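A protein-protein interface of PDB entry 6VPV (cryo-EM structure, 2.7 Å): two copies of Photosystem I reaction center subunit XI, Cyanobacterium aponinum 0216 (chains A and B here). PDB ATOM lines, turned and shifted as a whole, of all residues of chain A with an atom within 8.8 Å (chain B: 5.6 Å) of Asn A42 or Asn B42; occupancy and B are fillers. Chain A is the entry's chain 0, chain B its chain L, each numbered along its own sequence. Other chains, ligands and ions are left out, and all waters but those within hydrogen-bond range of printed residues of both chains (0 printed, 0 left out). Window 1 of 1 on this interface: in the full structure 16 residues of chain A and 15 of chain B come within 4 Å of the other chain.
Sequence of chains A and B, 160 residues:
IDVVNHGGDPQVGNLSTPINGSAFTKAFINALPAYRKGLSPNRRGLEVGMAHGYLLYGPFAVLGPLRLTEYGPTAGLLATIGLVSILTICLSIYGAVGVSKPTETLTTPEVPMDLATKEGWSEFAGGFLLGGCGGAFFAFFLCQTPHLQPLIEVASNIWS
ND2 of Asn B42 lies close to ND2 of Asn A42 (2.5 Å).
O of Glu B123 sits close to N of Asn B42, 3.4 Å away. OD1 of Asn B42 sits close to N of Gly B127, 3.5 Å away. The backbone NH (N) of Asn A42 lies close to the backbone carbonyl oxygen (O) of Glu A123 (3.4 Å). The side-chain amide oxygen (OD1) of Asn A42 sits close to the backbone NH (N) of Gly A127 (3.5 Å). NH2 of Arg A43 lies within salt-bridge range of OE1 of Glu A47 (3.7 Å).
Among the printed residues, pairs that only touch across the chains: Ser A40 with Glu B123, Leu A46 with Gly B126 and Arg A43 with Gly B126.
Asn A42 touches just one residue of chain B: Asn B42. Of the printed residues of chain B, Leu A46 touches Gly B126 (3.4 Å). Gly A131 touches none of the printed residues of chain B. Of chain A, only Asn A42 (2.5 Å) comes within 4 Å of Asn B42. Of the printed residues of chain A, Gly B126 touches Arg A43 (3.9 Å) and Leu A46 (3.4 Å). The nearest residue of chain A that does not touch Asn B42 is Pro A41 (5.7 Å). The nearest printed residue of chain B that does not touch Arg A43 is Glu B123 (4.7 Å).
Of the 25 printed residues of chain A, 4 touch a printed residue of chain B. Along chain A the printed residues that touch a printed residue of chain B span positions 40 to 46. Among the printed residues, 4 pairs touch across the chains.
Ser A40 touches Glu B123, but with the chains exchanged Glu A123 does not touch Ser B40 (9.0 Å). Asn A42 touches its own counterpart, Asn B42. Arg A43 touches Gly B126, but with the chains exchanged Gly A126 does not touch Arg B43 (12.9 Å). Leu A46 touches Gly B126, but with the chains exchanged Gly A126 does not touch Leu B46 (11.1 Å).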
ATOM      1  N   LEU A  39      10.672 -19.023  -9.034  1.00  0.00           N
ATOM      2  CA  LEU A  39       9.501 -18.915  -8.172  1.00  0.00           C
ATOM      3  C   LEU A  39       8.624 -17.730  -8.546  1.00  0.00           C
ATOM      4  O   LEU A  39       9.111 -16.669  -8.945  1.00  0.00           O
ATOM      5  CB  LEU A  39       9.911 -18.812  -6.702  1.00  0.00           C
ATOM      6  CG  LEU A  39      10.332 -20.056  -5.919  1.00  0.00           C
ATOM      7  CD1 LEU A  39      11.661 -20.598  -6.330  1.00  0.00           C
ATOM      8  CD2 LEU A  39      10.377 -19.687  -4.450  1.00  0.00           C
ATOM      9  N   SER A  40       7.334 -17.932  -8.422  1.00  0.00           N
ATOM     10  CA  SER A  40       6.324 -16.894  -8.510  1.00  0.00           C
ATOM     11  C   SER A  40       6.054 -16.337  -7.114  1.00  0.00           C
ATOM     12  O   SER A  40       6.416 -16.967  -6.119  1.00  0.00           O
ATOM     13  CB  SER A  40       5.037 -17.464  -9.104  1.00  0.00           C
ATOM     14  OG  SER A  40       4.395 -18.324  -8.178  1.00  0.00           O
ATOM     15  N   PRO A  41       5.440 -15.160  -7.003  1.00  0.00           N
ATOM     16  CA  PRO A  41       4.881 -14.753  -5.711  1.00  0.00           C
ATOM     17  C   PRO A  41       3.721 -15.664  -5.338  1.00  0.00           C
ATOM     18  O   PRO A  41       3.140 -16.328  -6.204  1.00  0.00           O
ATOM     19  CB  PRO A  41       4.426 -13.311  -5.956  1.00  0.00           C
ATOM     20  CG  PRO A  41       4.320 -13.184  -7.431  1.00  0.00           C
ATOM     21  CD  PRO A  41       5.385 -14.063  -7.982  1.00  0.00           C
ATOM     22  N   ASN A  42       3.425 -15.711  -4.025  1.00  0.00           N
ATOM     23  CA  ASN A  42       2.573 -16.661  -3.292  1.00  0.00           C
ATOM     24  C   ASN A  42       3.295 -18.007  -3.202  1.00  0.00           C
ATOM     25  O   ASN A  42       2.719 -19.017  -2.785  1.00  0.00           O
ATOM     26  CB  ASN A  42       1.165 -16.786  -3.914  1.00  0.00           C
ATOM     27  CG  ASN A  42       0.136 -17.372  -2.966  1.00  0.00           C
ATOM     28  OD1 ASN A  42       0.427 -17.675  -1.814  1.00  0.00           O
ATOM     29  ND2 ASN A  42      -1.086 -17.528  -3.458  1.00  0.00           N
ATOM     30  N   ARG A  43       4.569 -18.026  -3.597  1.00  0.00           N
ATOM     31  CA  ARG A  43       5.442 -19.157  -3.310  1.00  0.00           C
ATOM     32  C   ARG A  43       6.702 -18.684  -2.592  1.00  0.00           C
ATOM     33  O   ARG A  43       7.141 -19.305  -1.612  1.00  0.00           O
ATOM     34  CB  ARG A  43       5.777 -19.886  -4.609  1.00  0.00           C
ATOM     35  CG  ARG A  43       6.878 -20.910  -4.504  1.00  0.00           C
ATOM     36  CD  ARG A  43       6.497 -22.073  -3.614  1.00  0.00           C
ATOM     37  NE  ARG A  43       7.474 -23.151  -3.721  1.00  0.00           N
ATOM     38  CZ  ARG A  43       8.613 -23.197  -3.042  1.00  0.00           C
ATOM     39  NH1 ARG A  43       8.923 -22.233  -2.189  1.00  0.00           N
ATOM     40  NH2 ARG A  43       9.440 -24.216  -3.210  1.00  0.00           N
ATOM     41  N   ARG A  44       7.272 -17.566  -3.058  1.00  0.00           N
ATOM     42  CA  ARG A  44       8.298 -16.857  -2.302  1.00  0.00           C
ATOM     43  C   ARG A  44       7.764 -16.429  -0.947  1.00  0.00           C
ATOM     44  O   ARG A  44       8.418 -16.621   0.086  1.00  0.00           O
ATOM     45  CB  ARG A  44       8.759 -15.619  -3.070  1.00  0.00           C
ATOM     46  CG  ARG A  44       9.210 -15.833  -4.491  1.00  0.00           C
ATOM     47  CD  ARG A  44       9.768 -14.526  -5.028  1.00  0.00           C
ATOM     48  NE  ARG A  44       9.918 -14.524  -6.477  1.00  0.00           N
ATOM     49  CZ  ARG A  44      11.003 -14.949  -7.109  1.00  0.00           C
ATOM     50  NH1 ARG A  44      12.038 -15.405  -6.420  1.00  0.00           N
ATOM     51  NH2 ARG A  44      11.058 -14.915  -8.431  1.00  0.00           N
ATOM     52  N   GLY A  45       6.565 -15.842  -0.944  1.00  0.00           N
ATOM     53  CA  GLY A  45       5.949 -15.429   0.303  1.00  0.00           C
ATOM     54  C   GLY A  45       5.608 -16.606   1.193  1.00  0.00           C
ATOM     55  O   GLY A  45       5.715 -16.516   2.413  1.00  0.00           O
ATOM     56  N   LEU A  46       5.225 -17.734   0.587  1.00  0.00           N
ATOM     57  CA  LEU A  46       4.924 -18.940   1.354  1.00  0.00           C
ATOM     58  C   LEU A  46       6.158 -19.466   2.073  1.00  0.00           C
ATOM     59  O   LEU A  46       6.113 -19.764   3.271  1.00  0.00           O
ATOM     60  CB  LEU A  46       4.349 -20.012   0.429  1.00  0.00           C
ATOM     61  CG  LEU A  46       3.930 -21.323   1.090  1.00  0.00           C
ATOM     62  CD1 LEU A  46       2.792 -21.091   2.064  1.00  0.00           C
ATOM     63  CD2 LEU A  46       3.543 -22.343   0.039  1.00  0.00           C
ATOM     64  N   GLU A  47       7.284 -19.547   1.359  1.00  0.00           N
ATOM     65  CA  GLU A  47       8.525 -20.033   1.959  1.00  0.00           C
ATOM     66  C   GLU A  47       9.045 -19.075   3.030  1.00  0.00           C
ATOM     67  O   GLU A  47       9.444 -19.502   4.127  1.00  0.00           O
ATOM     68  CB  GLU A  47       9.564 -20.231   0.863  1.00  0.00           C
ATOM     69  CG  GLU A  47      10.678 -21.182   1.189  1.00  0.00           C
ATOM     70  CD  GLU A  47      11.520 -21.470  -0.029  1.00  0.00           C
ATOM     71  OE1 GLU A  47      10.950 -21.580  -1.132  1.00  0.00           O
ATOM     72  OE2 GLU A  47      12.755 -21.542   0.104  1.00  0.00           O
ATOM     73  N   VAL A  48       9.028 -17.770   2.727  1.00  0.00           N
ATOM     74  CA  VAL A  48       9.502 -16.751   3.663  1.00  0.00           C
ATOM     75  C   VAL A  48       8.637 -16.736   4.919  1.00  0.00           C
ATOM     76  O   VAL A  48       9.147 -16.705   6.046  1.00  0.00           O
ATOM     77  CB  VAL A  48       9.528 -15.376   2.971  1.00  0.00           C
ATOM     78  CG1 VAL A  48       9.558 -14.248   3.977  1.00  0.00           C
ATOM     79  CG2 VAL A  48      10.720 -15.274   2.051  1.00  0.00           C
ATOM     80  N   ASP A 114       8.619  -9.933 -10.819  1.00  0.00           N
ATOM     81  CA  ASP A 114       7.260 -10.181 -10.369  1.00  0.00           C
ATOM     82  C   ASP A 114       6.923  -9.468  -9.068  1.00  0.00           C
ATOM     83  O   ASP A 114       5.740  -9.314  -8.757  1.00  0.00           O
ATOM     84  CB  ASP A 114       7.027 -11.685 -10.206  1.00  0.00           C
ATOM     85  CG  ASP A 114       6.719 -12.373 -11.523  1.00  0.00           C
ATOM     86  OD1 ASP A 114       6.804 -11.708 -12.578  1.00  0.00           O
ATOM     87  OD2 ASP A 114       6.386 -13.576 -11.503  1.00  0.00           O
ATOM     88  N   LEU A 115       7.923  -9.029  -8.310  1.00  0.00           N
ATOM     89  CA  LEU A 115       7.704  -8.229  -7.115  1.00  0.00           C
ATOM     90  C   LEU A 115       7.754  -6.734  -7.393  1.00  0.00           C
ATOM     91  O   LEU A 115       7.681  -5.939  -6.452  1.00  0.00           O
ATOM     92  CB  LEU A 115       8.737  -8.582  -6.041  1.00  0.00           C
ATOM     93  CG  LEU A 115       8.586  -9.943  -5.365  1.00  0.00           C
ATOM     94  CD1 LEU A 115       9.716 -10.173  -4.380  1.00  0.00           C
ATOM     95  CD2 LEU A 115       7.243 -10.052  -4.674  1.00  0.00           C
ATOM     96  N   GLU A 119       0.348  -6.170  -7.868  1.00  0.00           N
ATOM     97  CA  GLU A 119      -0.312  -7.471  -7.849  1.00  0.00           C
ATOM     98  C   GLU A 119       0.627  -8.564  -7.358  1.00  0.00           C
ATOM     99  O   GLU A 119       0.189  -9.507  -6.693  1.00  0.00           O
ATOM    100  CB  GLU A 119      -0.846  -7.807  -9.240  1.00  0.00           C
ATOM    101  CG  GLU A 119      -2.092  -7.031  -9.633  1.00  0.00           C
ATOM    102  CD  GLU A 119      -1.772  -5.691 -10.267  1.00  0.00           C
ATOM    103  OE1 GLU A 119      -0.580  -5.422 -10.529  1.00  0.00           O
ATOM    104  OE2 GLU A 119      -2.713  -4.907 -10.506  1.00  0.00           O
ATOM    105  N   GLY A 120       1.915  -8.462  -7.686  1.00  0.00           N
ATOM    106  CA  GLY A 120       2.874  -9.438  -7.195  1.00  0.00           C
ATOM    107  C   GLY A 120       3.100  -9.341  -5.700  1.00  0.00           C
ATOM    108  O   GLY A 120       3.223 -10.357  -5.011  1.00  0.00           O
ATOM    109  N   TRP A 121       3.151  -8.119  -5.174  1.00  0.00           N
ATOM    110  CA  TRP A 121       3.310  -7.932  -3.740  1.00  0.00           C
ATOM    111  C   TRP A 121       2.060  -8.297  -2.952  1.00  0.00           C
ATOM    112  O   TRP A 121       2.158  -8.538  -1.746  1.00  0.00           O
ATOM    113  CB  TRP A 121       3.710  -6.490  -3.436  1.00  0.00           C
ATOM    114  CG  TRP A 121       4.635  -6.402  -2.279  1.00  0.00           C
ATOM    115  CD1 TRP A 121       4.294  -6.326  -0.963  1.00  0.00           C
ATOM    116  CD2 TRP A 121       6.065  -6.417  -2.323  1.00  0.00           C
ATOM    117  NE1 TRP A 121       5.423  -6.277  -0.185  1.00  0.00           N
ATOM    118  CE2 TRP A 121       6.524  -6.334  -0.996  1.00  0.00           C
ATOM    119  CE3 TRP A 121       7.001  -6.485  -3.357  1.00  0.00           C
ATOM    120  CZ2 TRP A 121       7.877  -6.319  -0.676  1.00  0.00           C
ATOM    121  CZ3 TRP A 121       8.344  -6.469  -3.037  1.00  0.00           C
ATOM    122  CH2 TRP A 121       8.770  -6.386  -1.707  1.00  0.00           C
ATOM    123  N   SER A 122       0.891  -8.333  -3.596  1.00  0.00           N
ATOM    124  CA  SER A 122      -0.299  -8.844  -2.926  1.00  0.00           C
ATOM    125  C   SER A 122      -0.242 -10.359  -2.794  1.00  0.00           C
ATOM    126  O   SER A 122      -0.618 -10.913  -1.752  1.00  0.00           O
ATOM    127  CB  SER A 122      -1.550  -8.415  -3.686  1.00  0.00           C
ATOM    128  OG  SER A 122      -1.777  -7.027  -3.535  1.00  0.00           O
ATOM    129  N   GLU A 123       0.226 -11.045  -3.842  1.00  0.00           N
ATOM    130  CA  GLU A 123       0.450 -12.482  -3.757  1.00  0.00           C
ATOM    131  C   GLU A 123       1.527 -12.819  -2.741  1.00  0.00           C
ATOM    132  O   GLU A 123       1.399 -13.813  -2.017  1.00  0.00           O
ATOM    133  CB  GLU A 123       0.829 -13.047  -5.126  1.00  0.00           C
ATOM    134  CG  GLU A 123      -0.150 -12.724  -6.235  1.00  0.00           C
ATOM    135  CD  GLU A 123       0.349 -13.168  -7.596  1.00  0.00           C
ATOM    136  OE1 GLU A 123       0.962 -14.252  -7.682  1.00  0.00           O
ATOM    137  OE2 GLU A 123       0.130 -12.431  -8.581  1.00  0.00           O
ATOM    138  N   PHE A 124       2.583 -12.003  -2.668  1.00  0.00           N
ATOM    139  CA  PHE A 124       3.623 -12.198  -1.663  1.00  0.00           C
ATOM    140  C   PHE A 124       3.064 -12.040  -0.254  1.00  0.00           C
ATOM    141  O   PHE A 124       3.406 -12.809   0.648  1.00  0.00           O
ATOM    142  CB  PHE A 124       4.771 -11.216  -1.899  1.00  0.00           C
ATOM    143  CG  PHE A 124       6.012 -11.535  -1.115  1.00  0.00           C
ATOM    144  CD1 PHE A 124       6.948 -12.425  -1.613  1.00  0.00           C
ATOM    145  CD2 PHE A 124       6.244 -10.950   0.119  1.00  0.00           C
ATOM    146  CE1 PHE A 124       8.088 -12.722  -0.898  1.00  0.00           C
ATOM    147  CE2 PHE A 124       7.381 -11.249   0.839  1.00  0.00           C
ATOM    148  CZ  PHE A 124       8.303 -12.133   0.330  1.00  0.00           C
ATOM    149  N   ALA A 125       2.189 -11.051  -0.052  1.00  0.00           N
ATOM    150  CA  ALA A 125       1.590 -10.836   1.262  1.00  0.00           C
ATOM    151  C   ALA A 125       0.651 -11.975   1.653  1.00  0.00           C
ATOM    152  O   ALA A 125       0.640 -12.410   2.810  1.00  0.00           O
ATOM    153  CB  ALA A 125       0.847  -9.501   1.284  1.00  0.00           C
ATOM    154  N   GLY A 126      -0.141 -12.468   0.699  1.00  0.00           N
ATOM    155  CA  GLY A 126      -1.022 -13.592   0.991  1.00  0.00           C
ATOM    156  C   GLY A 126      -0.256 -14.868   1.289  1.00  0.00           C
ATOM    157  O   GLY A 126      -0.603 -15.619   2.212  1.00  0.00           O
ATOM    158  N   GLY A 127       0.804 -15.123   0.518  1.00  0.00           N
ATOM    159  CA  GLY A 127       1.679 -16.239   0.813  1.00  0.00           C
ATOM    160  C   GLY A 127       2.382 -16.104   2.143  1.00  0.00           C
ATOM    161  O   GLY A 127       2.571 -17.099   2.844  1.00  0.00           O
ATOM    162  N   PHE A 128       2.751 -14.877   2.522  1.00  0.00           N
ATOM    163  CA  PHE A 128       3.347 -14.645   3.830  1.00  0.00           C
ATOM    164  C   PHE A 128       2.356 -14.935   4.946  1.00  0.00           C
ATOM    165  O   PHE A 128       2.733 -15.487   5.982  1.00  0.00           O
ATOM    166  CB  PHE A 128       3.864 -13.211   3.935  1.00  0.00           C
ATOM    167  CG  PHE A 128       4.594 -12.929   5.216  1.00  0.00           C
ATOM    168  CD1 PHE A 128       3.962 -12.293   6.272  1.00  0.00           C
ATOM    169  CD2 PHE A 128       5.913 -13.312   5.368  1.00  0.00           C
ATOM    170  CE1 PHE A 128       4.633 -12.048   7.450  1.00  0.00           C
ATOM    171  CE2 PHE A 128       6.588 -13.071   6.544  1.00  0.00           C
ATOM    172  CZ  PHE A 128       5.949 -12.436   7.586  1.00  0.00           C
ATOM    173  N   LEU A 129       1.085 -14.569   4.752  1.00  0.00           N
ATOM    174  CA  LEU A 129       0.061 -14.864   5.754  1.00  0.00           C
ATOM    175  C   LEU A 129      -0.122 -16.362   5.945  1.00  0.00           C
ATOM    176  O   LEU A 129      -0.083 -16.867   7.075  1.00  0.00           O
ATOM    177  CB  LEU A 129      -1.271 -14.235   5.357  1.00  0.00           C
ATOM    178  CG  LEU A 129      -2.385 -14.443   6.383  1.00  0.00           C
ATOM    179  CD1 LEU A 129      -2.034 -13.781   7.702  1.00  0.00           C
ATOM    180  CD2 LEU A 129      -3.708 -13.927   5.852  1.00  0.00           C
ATOM    181  N   LEU A 130      -0.323 -17.088   4.836  1.00  0.00           N
ATOM    182  CA  LEU A 130      -0.522 -18.534   4.925  1.00  0.00           C
ATOM    183  C   LEU A 130       0.713 -19.248   5.457  1.00  0.00           C
ATOM    184  O   LEU A 130       0.592 -20.134   6.312  1.00  0.00           O
ATOM    185  CB  LEU A 130      -0.929 -19.117   3.570  1.00  0.00           C
ATOM    186  CG  LEU A 130      -2.400 -19.093   3.128  1.00  0.00           C
ATOM    187  CD1 LEU A 130      -3.222 -19.951   4.077  1.00  0.00           C
ATOM    188  CD2 LEU A 130      -3.016 -17.709   3.003  1.00  0.00           C
ATOM    189  N   GLY A 131       1.901 -18.849   5.009  1.00  0.00           N
ATOM    190  CA  GLY A 131       3.136 -19.409   5.505  1.00  0.00           C
ATOM    191  C   GLY A 131       3.396 -19.121   6.966  1.00  0.00           C
ATOM    192  O   GLY A 131       3.822 -20.018   7.686  1.00  0.00           O
ATOM    193  N   SER B  40      -6.092 -22.309 -12.539  1.00  0.00           N
ATOM    194  CA  SER B  40      -4.728 -21.817 -12.494  1.00  0.00           C
ATOM    195  C   SER B  40      -3.904 -22.699 -11.559  1.00  0.00           C
ATOM    196  O   SER B  40      -4.472 -23.447 -10.761  1.00  0.00           O
ATOM    197  CB  SER B  40      -4.709 -20.372 -12.000  1.00  0.00           C
ATOM    198  OG  SER B  40      -5.014 -20.309 -10.618  1.00  0.00           O
ATOM    199  N   PRO B  41      -2.576 -22.652 -11.640  1.00  0.00           N
ATOM    200  CA  PRO B  41      -1.763 -23.224 -10.562  1.00  0.00           C
ATOM    201  C   PRO B  41      -1.954 -22.419  -9.285  1.00  0.00           C
ATOM    202  O   PRO B  41      -2.390 -21.264  -9.331  1.00  0.00           O
ATOM    203  CB  PRO B  41      -0.333 -23.123 -11.100  1.00  0.00           C
ATOM    204  CG  PRO B  41      -0.396 -22.103 -12.177  1.00  0.00           C
ATOM    205  CD  PRO B  41      -1.744 -22.253 -12.785  1.00  0.00           C
ATOM    206  N   ASN B  42      -1.657 -23.071  -8.144  1.00  0.00           N
ATOM    207  CA  ASN B  42      -1.972 -22.710  -6.753  1.00  0.00           C
ATOM    208  C   ASN B  42      -3.469 -22.922  -6.512  1.00  0.00           C
ATOM    209  O   ASN B  42      -4.013 -22.530  -5.475  1.00  0.00           O
ATOM    210  CB  ASN B  42      -1.514 -21.279  -6.400  1.00  0.00           C
ATOM    211  CG  ASN B  42      -1.396 -21.032  -4.909  1.00  0.00           C
ATOM    212  OD1 ASN B  42      -1.622 -21.920  -4.094  1.00  0.00           O
ATOM    213  ND2 ASN B  42      -1.032 -19.809  -4.547  1.00  0.00           N
ATOM    214  N   ARG B  43      -4.143 -23.548  -7.479  1.00  0.00           N
ATOM    215  CA  ARG B  43      -5.493 -24.054  -7.264  1.00  0.00           C
ATOM    216  C   ARG B  43      -5.565 -25.535  -7.613  1.00  0.00           C
ATOM    217  O   ARG B  43      -6.163 -26.331  -6.871  1.00  0.00           O
ATOM    218  CB  ARG B  43      -6.481 -23.235  -8.091  1.00  0.00           C
ATOM    219  CG  ARG B  43      -7.873 -23.806  -8.178  1.00  0.00           C
ATOM    220  CD  ARG B  43      -8.571 -23.823  -6.835  1.00  0.00           C
ATOM    221  NE  ARG B  43      -9.983 -24.154  -6.988  1.00  0.00           N
ATOM    222  CZ  ARG B  43     -10.456 -25.390  -7.083  1.00  0.00           C
ATOM    223  NH1 ARG B  43      -9.634 -26.427  -7.027  1.00  0.00           N
ATOM    224  NH2 ARG B  43     -11.756 -25.591  -7.224  1.00  0.00           N
ATOM    225  N   ARG B  44      -4.931 -25.920  -8.727  1.00  0.00           N
ATOM    226  CA  ARG B  44      -4.681 -27.327  -9.020  1.00  0.00           C
ATOM    227  C   ARG B  44      -3.853 -27.964  -7.919  1.00  0.00           C
ATOM    228  O   ARG B  44      -4.171 -29.057  -7.433  1.00  0.00           O
ATOM    229  CB  ARG B  44      -3.938 -27.466 -10.347  1.00  0.00           C
ATOM    230  CG  ARG B  44      -4.552 -26.784 -11.542  1.00  0.00           C
ATOM    231  CD  ARG B  44      -3.758 -27.161 -12.781  1.00  0.00           C
ATOM    232  NE  ARG B  44      -4.047 -26.306 -13.923  1.00  0.00           N
ATOM    233  CZ  ARG B  44      -5.022 -26.536 -14.793  1.00  0.00           C
ATOM    234  NH1 ARG B  44      -5.800 -27.598 -14.653  1.00  0.00           N
ATOM    235  NH2 ARG B  44      -5.218 -25.706 -15.805  1.00  0.00           N
ATOM    236  N   GLY B  45      -2.779 -27.281  -7.519  1.00  0.00           N
ATOM    237  CA  GLY B  45      -1.942 -27.784  -6.446  1.00  0.00           C
ATOM    238  C   GLY B  45      -2.670 -27.826  -5.119  1.00  0.00           C
ATOM    239  O   GLY B  45      -2.456 -28.735  -4.320  1.00  0.00           O
ATOM    240  N   LEU B  46      -3.563 -26.860  -4.887  1.00  0.00           N
ATOM    241  CA  LEU B  46      -4.354 -26.840  -3.659  1.00  0.00           C
ATOM    242  C   LEU B  46      -5.282 -28.044  -3.575  1.00  0.00           C
ATOM    243  O   LEU B  46      -5.338 -28.728  -2.547  1.00  0.00           O
ATOM    244  CB  LEU B  46      -5.156 -25.542  -3.580  1.00  0.00           C
ATOM    245  CG  LEU B  46      -5.999 -25.342  -2.323  1.00  0.00           C
ATOM    246  CD1 LEU B  46      -5.116 -25.252  -1.095  1.00  0.00           C
ATOM    247  CD2 LEU B  46      -6.865 -24.106  -2.459  1.00  0.00           C
ATOM    248  N   GLY B 120       4.802 -21.490 -13.046  1.00  0.00           N
ATOM    249  CA  GLY B 120       3.576 -22.231 -12.793  1.00  0.00           C
ATOM    250  C   GLY B 120       3.782 -23.407 -11.860  1.00  0.00           C
ATOM    251  O   GLY B 120       2.945 -23.683 -10.996  1.00  0.00           O
ATOM    252  N   GLU B 123       3.932 -22.177  -8.242  1.00  0.00           N
ATOM    253  CA  GLU B 123       2.589 -22.012  -7.700  1.00  0.00           C
ATOM    254  C   GLU B 123       1.943 -23.353  -7.393  1.00  0.00           C
ATOM    255  O   GLU B 123       1.251 -23.482  -6.378  1.00  0.00           O
ATOM    256  CB  GLU B 123       1.713 -21.222  -8.670  1.00  0.00           C
ATOM    257  CG  GLU B 123       2.285 -19.886  -9.092  1.00  0.00           C
ATOM    258  CD  GLU B 123       1.459 -19.216 -10.172  1.00  0.00           C
ATOM    259  OE1 GLU B 123       0.215 -19.303 -10.111  1.00  0.00           O
ATOM    260  OE2 GLU B 123       2.053 -18.602 -11.084  1.00  0.00           O
ATOM    261  N   PHE B 124       2.169 -24.355  -8.247  1.00  0.00           N
ATOM    262  CA  PHE B 124       1.663 -25.700  -7.988  1.00  0.00           C
ATOM    263  C   PHE B 124       2.277 -26.284  -6.721  1.00  0.00           C
ATOM    264  O   PHE B 124       1.584 -26.921  -5.923  1.00  0.00           O
ATOM    265  CB  PHE B 124       1.942 -26.606  -9.188  1.00  0.00           C
ATOM    266  CG  PHE B 124       1.200 -27.911  -9.147  1.00  0.00           C
ATOM    267  CD1 PHE B 124      -0.089 -28.002  -9.642  1.00  0.00           C
ATOM    268  CD2 PHE B 124       1.788 -29.047  -8.611  1.00  0.00           C
ATOM    269  CE1 PHE B 124      -0.775 -29.198  -9.606  1.00  0.00           C
ATOM    270  CE2 PHE B 124       1.103 -30.242  -8.569  1.00  0.00           C
ATOM    271  CZ  PHE B 124      -0.177 -30.317  -9.067  1.00  0.00           C
ATOM    272  N   GLY B 126       3.554 -24.558  -4.122  1.00  0.00           N
ATOM    273  CA  GLY B 126       3.035 -23.840  -2.966  1.00  0.00           C
ATOM    274  C   GLY B 126       1.611 -24.238  -2.626  1.00  0.00           C
ATOM    275  O   GLY B 126       1.261 -24.411  -1.449  1.00  0.00           O
ATOM    276  N   GLY B 127       0.774 -24.402  -3.653  1.00  0.00           N
ATOM    277  CA  GLY B 127      -0.563 -24.917  -3.441  1.00  0.00           C
ATOM    278  C   GLY B 127      -0.574 -26.328  -2.900  1.00  0.00           C
ATOM    279  O   GLY B 127      -1.422 -26.663  -2.073  1.00  0.00           O
